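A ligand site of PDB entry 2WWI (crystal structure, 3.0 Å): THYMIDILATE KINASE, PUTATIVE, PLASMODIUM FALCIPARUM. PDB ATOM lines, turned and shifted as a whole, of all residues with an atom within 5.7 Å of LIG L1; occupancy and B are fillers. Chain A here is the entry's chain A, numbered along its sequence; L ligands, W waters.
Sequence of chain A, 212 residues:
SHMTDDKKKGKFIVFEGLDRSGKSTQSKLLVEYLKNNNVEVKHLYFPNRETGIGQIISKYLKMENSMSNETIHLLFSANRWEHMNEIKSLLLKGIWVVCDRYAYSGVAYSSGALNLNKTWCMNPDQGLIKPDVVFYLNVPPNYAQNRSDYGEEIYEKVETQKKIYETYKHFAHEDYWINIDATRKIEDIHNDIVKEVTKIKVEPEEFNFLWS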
ATOM      1  N   LEU A  18      10.378  11.218  -7.427  1.00  0.00           N
ATOM      2  CA  LEU A  18       9.123  10.664  -7.906  1.00  0.00           C
ATOM      3  C   LEU A  18       9.245  10.440  -9.379  1.00  0.00           C
ATOM      4  O   LEU A  18      10.240  10.828 -10.025  1.00  0.00           O
ATOM      5  CB  LEU A  18       7.930  11.567  -7.584  1.00  0.00           C
ATOM      6  CG  LEU A  18       7.413  11.583  -6.128  1.00  0.00           C
ATOM      7  CD1 LEU A  18       6.121  12.322  -6.041  1.00  0.00           C
ATOM      8  CD2 LEU A  18       7.198  10.199  -5.579  1.00  0.00           C
ATOM      9  N   ASP A  19       8.252   9.768  -9.930  1.00  0.00           N
ATOM     10  CA  ASP A  19       8.329   9.391 -11.307  1.00  0.00           C
ATOM     11  C   ASP A  19       8.218  10.638 -12.120  1.00  0.00           C
ATOM     12  O   ASP A  19       7.691  11.624 -11.648  1.00  0.00           O
ATOM     13  CB  ASP A  19       7.246   8.386 -11.642  1.00  0.00           C
ATOM     14  CG  ASP A  19       7.670   6.993 -11.269  1.00  0.00           C
ATOM     15  OD1 ASP A  19       8.186   6.286 -12.176  1.00  0.00           O
ATOM     16  OD2 ASP A  19       7.546   6.637 -10.066  1.00  0.00           O
ATOM     17  N   ARG A  20       8.783  10.624 -13.317  1.00  0.00           N
ATOM     18  CA  ARG A  20       8.707  11.776 -14.202  1.00  0.00           C
ATOM     19  C   ARG A  20       9.157  13.099 -13.518  1.00  0.00           C
ATOM     20  O   ARG A  20       8.680  14.186 -13.857  1.00  0.00           O
ATOM     21  CB  ARG A  20       7.283  11.882 -14.808  1.00  0.00           C
ATOM     22  CG  ARG A  20       7.087  11.147 -16.142  1.00  0.00           C
ATOM     23  CD  ARG A  20       7.347   9.642 -16.076  1.00  0.00           C
ATOM     24  NE  ARG A  20       7.696   9.045 -17.375  1.00  0.00           N
ATOM     25  CZ  ARG A  20       7.017   8.061 -17.973  1.00  0.00           C
ATOM     26  NH1 ARG A  20       5.938   7.539 -17.413  1.00  0.00           N
ATOM     27  NH2 ARG A  20       7.412   7.599 -19.145  1.00  0.00           N
ATOM     28  N   SER A  21      10.066  13.014 -12.543  1.00  0.00           N
ATOM     29  CA  SER A  21      10.586  14.232 -11.925  1.00  0.00           C
ATOM     30  C   SER A  21      11.927  14.767 -12.491  1.00  0.00           C
ATOM     31  O   SER A  21      12.586  15.601 -11.871  1.00  0.00           O
ATOM     32  CB  SER A  21      10.609  14.104 -10.395  1.00  0.00           C
ATOM     33  OG  SER A  21      11.599  13.203  -9.975  1.00  0.00           O
ATOM     34  N   GLY A  22      12.332  14.321 -13.674  1.00  0.00           N
ATOM     35  CA  GLY A  22      13.532  14.878 -14.295  1.00  0.00           C
ATOM     36  C   GLY A  22      14.850  14.252 -13.865  1.00  0.00           C
ATOM     37  O   GLY A  22      15.913  14.829 -14.120  1.00  0.00           O
ATOM     38  N   LYS A  23      14.786  13.090 -13.218  1.00  0.00           N
ATOM     39  CA  LYS A  23      15.999  12.311 -12.902  1.00  0.00           C
ATOM     40  C   LYS A  23      16.912  12.120 -14.127  1.00  0.00           C
ATOM     41  O   LYS A  23      18.100  12.467 -14.074  1.00  0.00           O
ATOM     42  CB  LYS A  23      15.653  10.981 -12.235  1.00  0.00           C
ATOM     43  CG  LYS A  23      15.113  11.123 -10.795  1.00  0.00           C
ATOM     44  CD  LYS A  23      14.682   9.801 -10.169  1.00  0.00           C
ATOM     45  CE  LYS A  23      13.219   9.501 -10.423  1.00  0.00           C
ATOM     46  NZ  LYS A  23      12.917   8.901 -11.762  1.00  0.00           N
ATOM     47  N   SER A  24      16.369  11.618 -15.229  1.00  0.00           N
ATOM     48  CA  SER A  24      17.168  11.431 -16.434  1.00  0.00           C
ATOM     49  C   SER A  24      17.790  12.756 -16.881  1.00  0.00           C
ATOM     50  O   SER A  24      19.022  12.907 -16.830  1.00  0.00           O
ATOM     51  CB  SER A  24      16.339  10.845 -17.572  1.00  0.00           C
ATOM     52  OG  SER A  24      15.735   9.635 -17.160  1.00  0.00           O
ATOM     53  N   THR A  25      16.932  13.697 -17.283  1.00  0.00           N
ATOM     54  CA  THR A  25      17.334  15.048 -17.665  1.00  0.00           C
ATOM     55  C   THR A  25      18.512  15.610 -16.859  1.00  0.00           C
ATOM     56  O   THR A  25      19.474  16.163 -17.423  1.00  0.00           O
ATOM     57  CB  THR A  25      16.154  16.034 -17.536  1.00  0.00           C
ATOM     58  OG1 THR A  25      14.962  15.449 -18.092  1.00  0.00           O
ATOM     59  CG2 THR A  25      16.461  17.344 -18.249  1.00  0.00           C
ATOM     60  N   GLN A  26      18.424  15.481 -15.539  1.00  0.00           N
ATOM     61  CA  GLN A  26      19.423  16.024 -14.650  1.00  0.00           C
ATOM     62  C   GLN A  26      20.662  15.149 -14.551  1.00  0.00           C
ATOM     63  O   GLN A  26      21.791  15.649 -14.519  1.00  0.00           O
ATOM     64  CB  GLN A  26      18.820  16.272 -13.270  1.00  0.00           C
ATOM     65  CG  GLN A  26      17.765  17.401 -13.261  1.00  0.00           C
ATOM     66  CD  GLN A  26      18.289  18.756 -13.732  1.00  0.00           C
ATOM     67  OE1 GLN A  26      19.491  19.066 -13.607  1.00  0.00           O
ATOM     68  NE2 GLN A  26      17.388  19.591 -14.270  1.00  0.00           N
ATOM     69  N   ASP A 100      21.095   6.867 -11.589  1.00  0.00           N
ATOM     70  CA  ASP A 100      19.794   7.380 -11.271  1.00  0.00           C
ATOM     71  C   ASP A 100      18.791   6.360 -10.765  1.00  0.00           C
ATOM     72  O   ASP A 100      18.469   5.388 -11.434  1.00  0.00           O
ATOM     73  CB  ASP A 100      19.325   8.453 -12.263  1.00  0.00           C
ATOM     74  CG  ASP A 100      18.458   7.922 -13.311  1.00  0.00           C
ATOM     75  OD1 ASP A 100      17.397   7.374 -12.947  1.00  0.00           O
ATOM     76  OD2 ASP A 100      18.820   8.105 -14.510  1.00  0.00           O
ATOM     77  N   ARG A 101      18.379   6.606  -9.516  1.00  0.00           N
ATOM     78  CA  ARG A 101      17.766   5.616  -8.604  1.00  0.00           C
ATOM     79  C   ARG A 101      18.789   4.649  -8.006  1.00  0.00           C
ATOM     80  O   ARG A 101      19.671   4.136  -8.707  1.00  0.00           O
ATOM     81  CB  ARG A 101      16.627   4.849  -9.261  1.00  0.00           C
ATOM     82  CG  ARG A 101      15.426   5.697  -9.577  1.00  0.00           C
ATOM     83  CD  ARG A 101      14.203   4.823  -9.766  1.00  0.00           C
ATOM     84  NE  ARG A 101      13.055   5.529 -10.319  1.00  0.00           N
ATOM     85  CZ  ARG A 101      12.238   6.327  -9.631  1.00  0.00           C
ATOM     86  NH1 ARG A 101      12.443   6.568  -8.346  1.00  0.00           N
ATOM     87  NH2 ARG A 101      11.202   6.900 -10.232  1.00  0.00           N
ATOM     88  N   LEU A 137      15.325  15.060  -6.275  1.00  0.00           N
ATOM     89  CA  LEU A 137      14.505  15.990  -7.050  1.00  0.00           C
ATOM     90  C   LEU A 137      13.116  16.004  -6.464  1.00  0.00           C
ATOM     91  O   LEU A 137      12.255  15.271  -6.918  1.00  0.00           O
ATOM     92  CB  LEU A 137      14.447  15.587  -8.533  1.00  0.00           C
ATOM     93  CG  LEU A 137      15.783  15.293  -9.250  1.00  0.00           C
ATOM     94  CD1 LEU A 137      15.618  15.221 -10.764  1.00  0.00           C
ATOM     95  CD2 LEU A 137      16.869  16.311  -8.872  1.00  0.00           C
ATOM     96  N   TYR A 143       2.203  16.996  -9.210  1.00  0.00           N
ATOM     97  CA  TYR A 143       2.923  17.892 -10.098  1.00  0.00           C
ATOM     98  C   TYR A 143       3.283  17.264 -11.435  1.00  0.00           C
ATOM     99  O   TYR A 143       3.107  17.890 -12.489  1.00  0.00           O
ATOM    100  CB  TYR A 143       4.214  18.318  -9.415  1.00  0.00           C
ATOM    101  CG  TYR A 143       5.122  19.161 -10.290  1.00  0.00           C
ATOM    102  CD1 TYR A 143       4.788  20.485 -10.597  1.00  0.00           C
ATOM    103  CD2 TYR A 143       6.319  18.637 -10.782  1.00  0.00           C
ATOM    104  CE1 TYR A 143       5.620  21.261 -11.386  1.00  0.00           C
ATOM    105  CE2 TYR A 143       7.152  19.425 -11.580  1.00  0.00           C
ATOM    106  CZ  TYR A 143       6.793  20.737 -11.871  1.00  0.00           C
ATOM    107  OH  TYR A 143       7.603  21.519 -12.632  1.00  0.00           O
ATOM    108  N   ARG A 147       3.579  15.633 -16.977  1.00  0.00           N
ATOM    109  CA  ARG A 147       4.768  15.341 -17.813  1.00  0.00           C
ATOM    110  C   ARG A 147       4.597  14.278 -18.892  1.00  0.00           C
ATOM    111  O   ARG A 147       3.819  13.351 -18.739  1.00  0.00           O
ATOM    112  CB  ARG A 147       5.951  14.924 -16.931  1.00  0.00           C
ATOM    113  CG  ARG A 147       6.322  15.906 -15.827  1.00  0.00           C
ATOM    114  CD  ARG A 147       7.514  16.752 -16.210  1.00  0.00           C
ATOM    115  NE  ARG A 147       8.400  16.993 -15.070  1.00  0.00           N
ATOM    116  CZ  ARG A 147       8.673  18.193 -14.569  1.00  0.00           C
ATOM    117  NH1 ARG A 147       9.496  18.293 -13.543  1.00  0.00           N
ATOM    118  NH2 ARG A 147       8.134  19.298 -15.083  1.00  0.00           N
ATOM    119  N   SER A 148       5.396  14.405 -19.930  1.00  0.00           N
ATOM    120  CA  SER A 148       5.528  13.436 -21.016  1.00  0.00           C
ATOM    121  C   SER A 148       4.602  12.216 -21.113  1.00  0.00           C
ATOM    122  O   SER A 148       3.588  12.253 -21.816  1.00  0.00           O
ATOM    123  N   ALA A 182      12.303  20.747  -7.545  1.00  0.00           N
ATOM    124  CA  ALA A 182      12.381  20.318  -8.919  1.00  0.00           C
ATOM    125  C   ALA A 182      11.221  20.791  -9.721  1.00  0.00           C
ATOM    126  O   ALA A 182      10.976  20.309 -10.826  1.00  0.00           O
ATOM    127  CB  ALA A 182      12.519  18.813  -9.016  1.00  0.00           C
ATOM    128  N   ARG A 184      11.042  23.743 -10.892  1.00  0.00           N
ATOM    129  CA  ARG A 184      11.564  24.933 -11.544  1.00  0.00           C
ATOM    130  C   ARG A 184      12.099  24.649 -12.938  1.00  0.00           C
ATOM    131  O   ARG A 184      12.063  23.498 -13.402  1.00  0.00           O
ATOM    132  CB  ARG A 184      12.673  25.536 -10.699  1.00  0.00           C
ATOM    133  CG  ARG A 184      12.204  26.044  -9.374  1.00  0.00           C
ATOM    134  CD  ARG A 184      13.379  26.545  -8.639  1.00  0.00           C
ATOM    135  NE  ARG A 184      14.128  25.448  -8.062  1.00  0.00           N
ATOM    136  CZ  ARG A 184      15.448  25.477  -7.839  1.00  0.00           C
ATOM    137  NH1 ARG A 184      16.168  26.538  -8.167  1.00  0.00           N
ATOM    138  NH2 ARG A 184      16.026  24.414  -7.309  1.00  0.00           N
ATOM    139  N   LYS A 185      12.592  25.706 -13.597  1.00  0.00           N
ATOM    140  CA  LYS A 185      13.264  25.609 -14.895  1.00  0.00           C
ATOM    141  C   LYS A 185      14.360  24.551 -14.780  1.00  0.00           C
ATOM    142  O   LYS A 185      14.946  24.376 -13.689  1.00  0.00           O
ATOM    143  N   ILE A 186      14.617  23.856 -15.882  1.00  0.00           N
ATOM    144  CA  ILE A 186      15.659  22.823 -15.945  1.00  0.00           C
ATOM    145  C   ILE A 186      17.036  23.349 -15.515  1.00  0.00           C
ATOM    146  O   ILE A 186      17.719  22.719 -14.701  1.00  0.00           O
ATOM    147  CB  ILE A 186      15.733  22.174 -17.328  1.00  0.00           C
ATOM    148  CG1 ILE A 186      14.516  21.264 -17.539  1.00  0.00           C
ATOM    149  CG2 ILE A 186      16.988  21.374 -17.467  1.00  0.00           C
ATOM    150  CD1 ILE A 186      14.042  21.053 -19.012  1.00  0.00           C
ATOM    151  N   ILE A 189      17.582  23.938 -11.779  1.00  0.00           N
ATOM    152  CA  ILE A 189      17.848  22.665 -11.100  1.00  0.00           C
ATOM    153  C   ILE A 189      19.289  22.295 -11.415  1.00  0.00           C
ATOM    154  O   ILE A 189      20.090  21.979 -10.506  1.00  0.00           O
ATOM    155  CB  ILE A 189      16.824  21.515 -11.474  1.00  0.00           C
ATOM    156  CG1 ILE A 189      15.402  21.875 -11.015  1.00  0.00           C
ATOM    157  CG2 ILE A 189      17.182  20.235 -10.777  1.00  0.00           C
ATOM    158  CD1 ILE A 189      14.309  21.398 -11.917  1.00  0.00           C
HETATM  159  P1  LIG L   1      12.628  10.881 -14.656  1.00  0.00           P
HETATM  160  O1  LIG L   1      13.923  10.451 -15.301  1.00  0.00           O
HETATM  161  O2  LIG L   1      12.780  11.399 -13.252  1.00  0.00           O
HETATM  162  O3  LIG L   1      11.524   9.889 -14.838  1.00  0.00           O
HETATM  163  P2  LIG L   1      12.742  12.624 -16.940  1.00  0.00           P
HETATM  164  O4  LIG L   1      14.109  13.212 -16.667  1.00  0.00           O
HETATM  165  O5  LIG L   1      12.625  11.552 -17.998  1.00  0.00           O
HETATM  166  O6  LIG L   1      12.089  12.131 -15.533  1.00  0.00           O
HETATM  167  O7  LIG L   1      11.687  13.748 -17.397  1.00  0.00           O
HETATM  168  C1  LIG L   1      10.313  13.382 -17.614  1.00  0.00           C
HETATM  169  C2  LIG L   1       9.682  14.226 -18.715  1.00  0.00           C
HETATM  170  O8  LIG L   1       9.464  15.518 -18.182  1.00  0.00           O
HETATM  171  C3  LIG L   1      10.619  14.389 -19.915  1.00  0.00           C
HETATM  172  O9  LIG L   1       9.910  14.414 -21.167  1.00  0.00           O
HETATM  173  C4  LIG L   1      11.289  15.724 -19.703  1.00  0.00           C
HETATM  174  O10 LIG L   1      11.476  16.344 -20.970  1.00  0.00           O
HETATM  175  C5  LIG L   1      10.285  16.478 -18.860  1.00  0.00           C
HETATM  176  N1  LIG L   1      10.930  17.365 -17.854  1.00  0.00           N
HETATM  177  C6  LIG L   1      11.892  16.987 -16.998  1.00  0.00           C
HETATM  178  N2  LIG L   1      12.266  18.024 -16.222  1.00  0.00           N
HETATM  179  C7  LIG L   1      11.530  19.086 -16.572  1.00  0.00           C
HETATM  180  C8  LIG L   1      11.434  20.493 -16.112  1.00  0.00           C
HETATM  181  N3  LIG L   1      12.244  20.922 -15.115  1.00  0.00           N
HETATM  182  N4  LIG L   1      10.526  21.294 -16.743  1.00  0.00           N
HETATM  183  C9  LIG L   1       9.732  20.843 -17.743  1.00  0.00           C
HETATM  184  N5  LIG L   1       9.778  19.573 -18.195  1.00  0.00           N
HETATM  185  C10 LIG L   1      10.638  18.657 -17.655  1.00  0.00           C
HETATM  186  P1  LG2 L   2      12.176   4.350 -13.870  1.00  0.00           P
HETATM  187  O1  LG2 L   2      11.232   5.507 -13.815  1.00  0.00           O
HETATM  188  O2  LG2 L   2      13.453   4.551 -12.934  1.00  0.00           O
HETATM  189  O3  LG2 L   2      12.800   4.159 -15.289  1.00  0.00           O
HETATM  190  O4  LG2 L   2      11.507   2.953 -13.458  1.00  0.00           O
HETATM  191  C1  LG2 L   2      11.646   2.501 -12.121  1.00  0.00           C
HETATM  192  C2  LG2 L   2      10.336   2.261 -11.455  1.00  0.00           C
HETATM  193  O5  LG2 L   2      10.696   1.289 -10.481  1.00  0.00           O
HETATM  194  C3  LG2 L   2       9.946   3.497 -10.676  1.00  0.00           C
HETATM  195  N1  LG2 L   2       8.474   3.673 -10.658  1.00  0.00           N
HETATM  196  N2  LG2 L   2       7.844   3.397 -11.585  1.00  0.00           N
HETATM  197  N3  LG2 L   2       7.117   3.145 -12.439  1.00  0.00           N
HETATM  198  C4  LG2 L   2      10.425   3.227  -9.237  1.00  0.00           C
HETATM  199  C5  LG2 L   2      10.408   1.739  -9.140  1.00  0.00           C
HETATM  200  N4  LG2 L   2      11.516   1.129  -8.374  1.00  0.00           N
HETATM  201  C6  LG2 L   2      11.273   0.316  -7.242  1.00  0.00           C
HETATM  202  O6  LG2 L   2      10.122   0.102  -6.855  1.00  0.00           O
HETATM  203  N5  LG2 L   2      12.289  -0.242  -6.554  1.00  0.00           N
HETATM  204  C7  LG2 L   2      13.544  -0.048  -6.950  1.00  0.00           C
HETATM  205  O7  LG2 L   2      14.532  -0.640  -6.229  1.00  0.00           O
HETATM  206  C8  LG2 L   2      13.827   0.721  -8.061  1.00  0.00           C
HETATM  207  C9  LG2 L   2      15.256   0.951  -8.518  1.00  0.00           C
HETATM  208  C10 LG2 L   2      12.813   1.312  -8.788  1.00  0.00           C
HETATM  209  O   HOH W   1       9.949  14.725 -24.198  1.00  0.00           O
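Arg 147 touches LIG L1 (CD to O8, 3.0 Å). Ile 186 touches LIG L1 (CG1 to N3, 3.3 Å). Ile 189 touches LIG L1. Ten residues have an atom within 4 Å of LIG L1: Arg 20, Ser 21, Gly 22, Lys 23, Ser 24, Thr 25, Arg 147, Arg 184, Ile 186 and Ile 189. Along chain A the residues within 4 Å of LIG L1 span positions 20 to 189. The nearest printed residue that does not touch LIG L1 is Leu 18 (4.1 Å).
The side-chain hydroxyl (OG) of Ser 24 sits at hydrogen-bond distance from an oxygen (O1) of LIG L1, at 2.7 Å. The backbone NH (N) of Lys 23 lies within hydrogen-bond range of an oxygen (O2) of LIG L1 (2.6 Å). The backbone NH of Arg 20 sits at hydrogen-bond distance from an oxygen (O3) of LIG L1, at 3.2 Å. The backbone carbonyl oxygen (O) of Arg 184 lies within hydrogen-bond range of a nitrogen (N3) of LIG L1. The backbone NH (N) of Ser 21 is in hydrogen-bond range of an oxygen (O2) of LIG L1, at 3.2 Å. The side-chain hydroxyl (OG1) of Thr 25 sits at hydrogen-bond distance from an oxygen (O4) of LIG L1. The backbone NH (N) of Gly 22 lies within hydrogen-bond range of an oxygen (O6) of LIG L1. An oxygen (O4) of LIG L1 sits at hydrogen-bond distance from the backbone NH (N) of Thr 25 (2.9 Å). The guanidinium group of Arg 101 lies within salt-bridge range of an oxygen (O2) of LG2 L2, 2.8 Å away. The backbone NH (N) of Ser 24 is in hydrogen-bond range of an oxygen (O1) of LIG L1 (2.7 Å). The side-chain amino group of Lys 23 is in salt-bridge range of an oxygen (O2) of LIG L1, 2.9 Å away.
NH2 of Arg 147 lies within hydrogen-bond range of OH of Tyr 143 (3.3 Å). The side-chain amide nitrogen of Gln 26 sits at hydrogen-bond distance from the backbone carbonyl oxygen of Ile 186 (3.2 Å). NE of Arg 147 sits at hydrogen-bond distance from O of Arg 20 (3.1 Å). O of Leu 18 is in hydrogen-bond range of OG of Ser 21 (2.7 Å).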
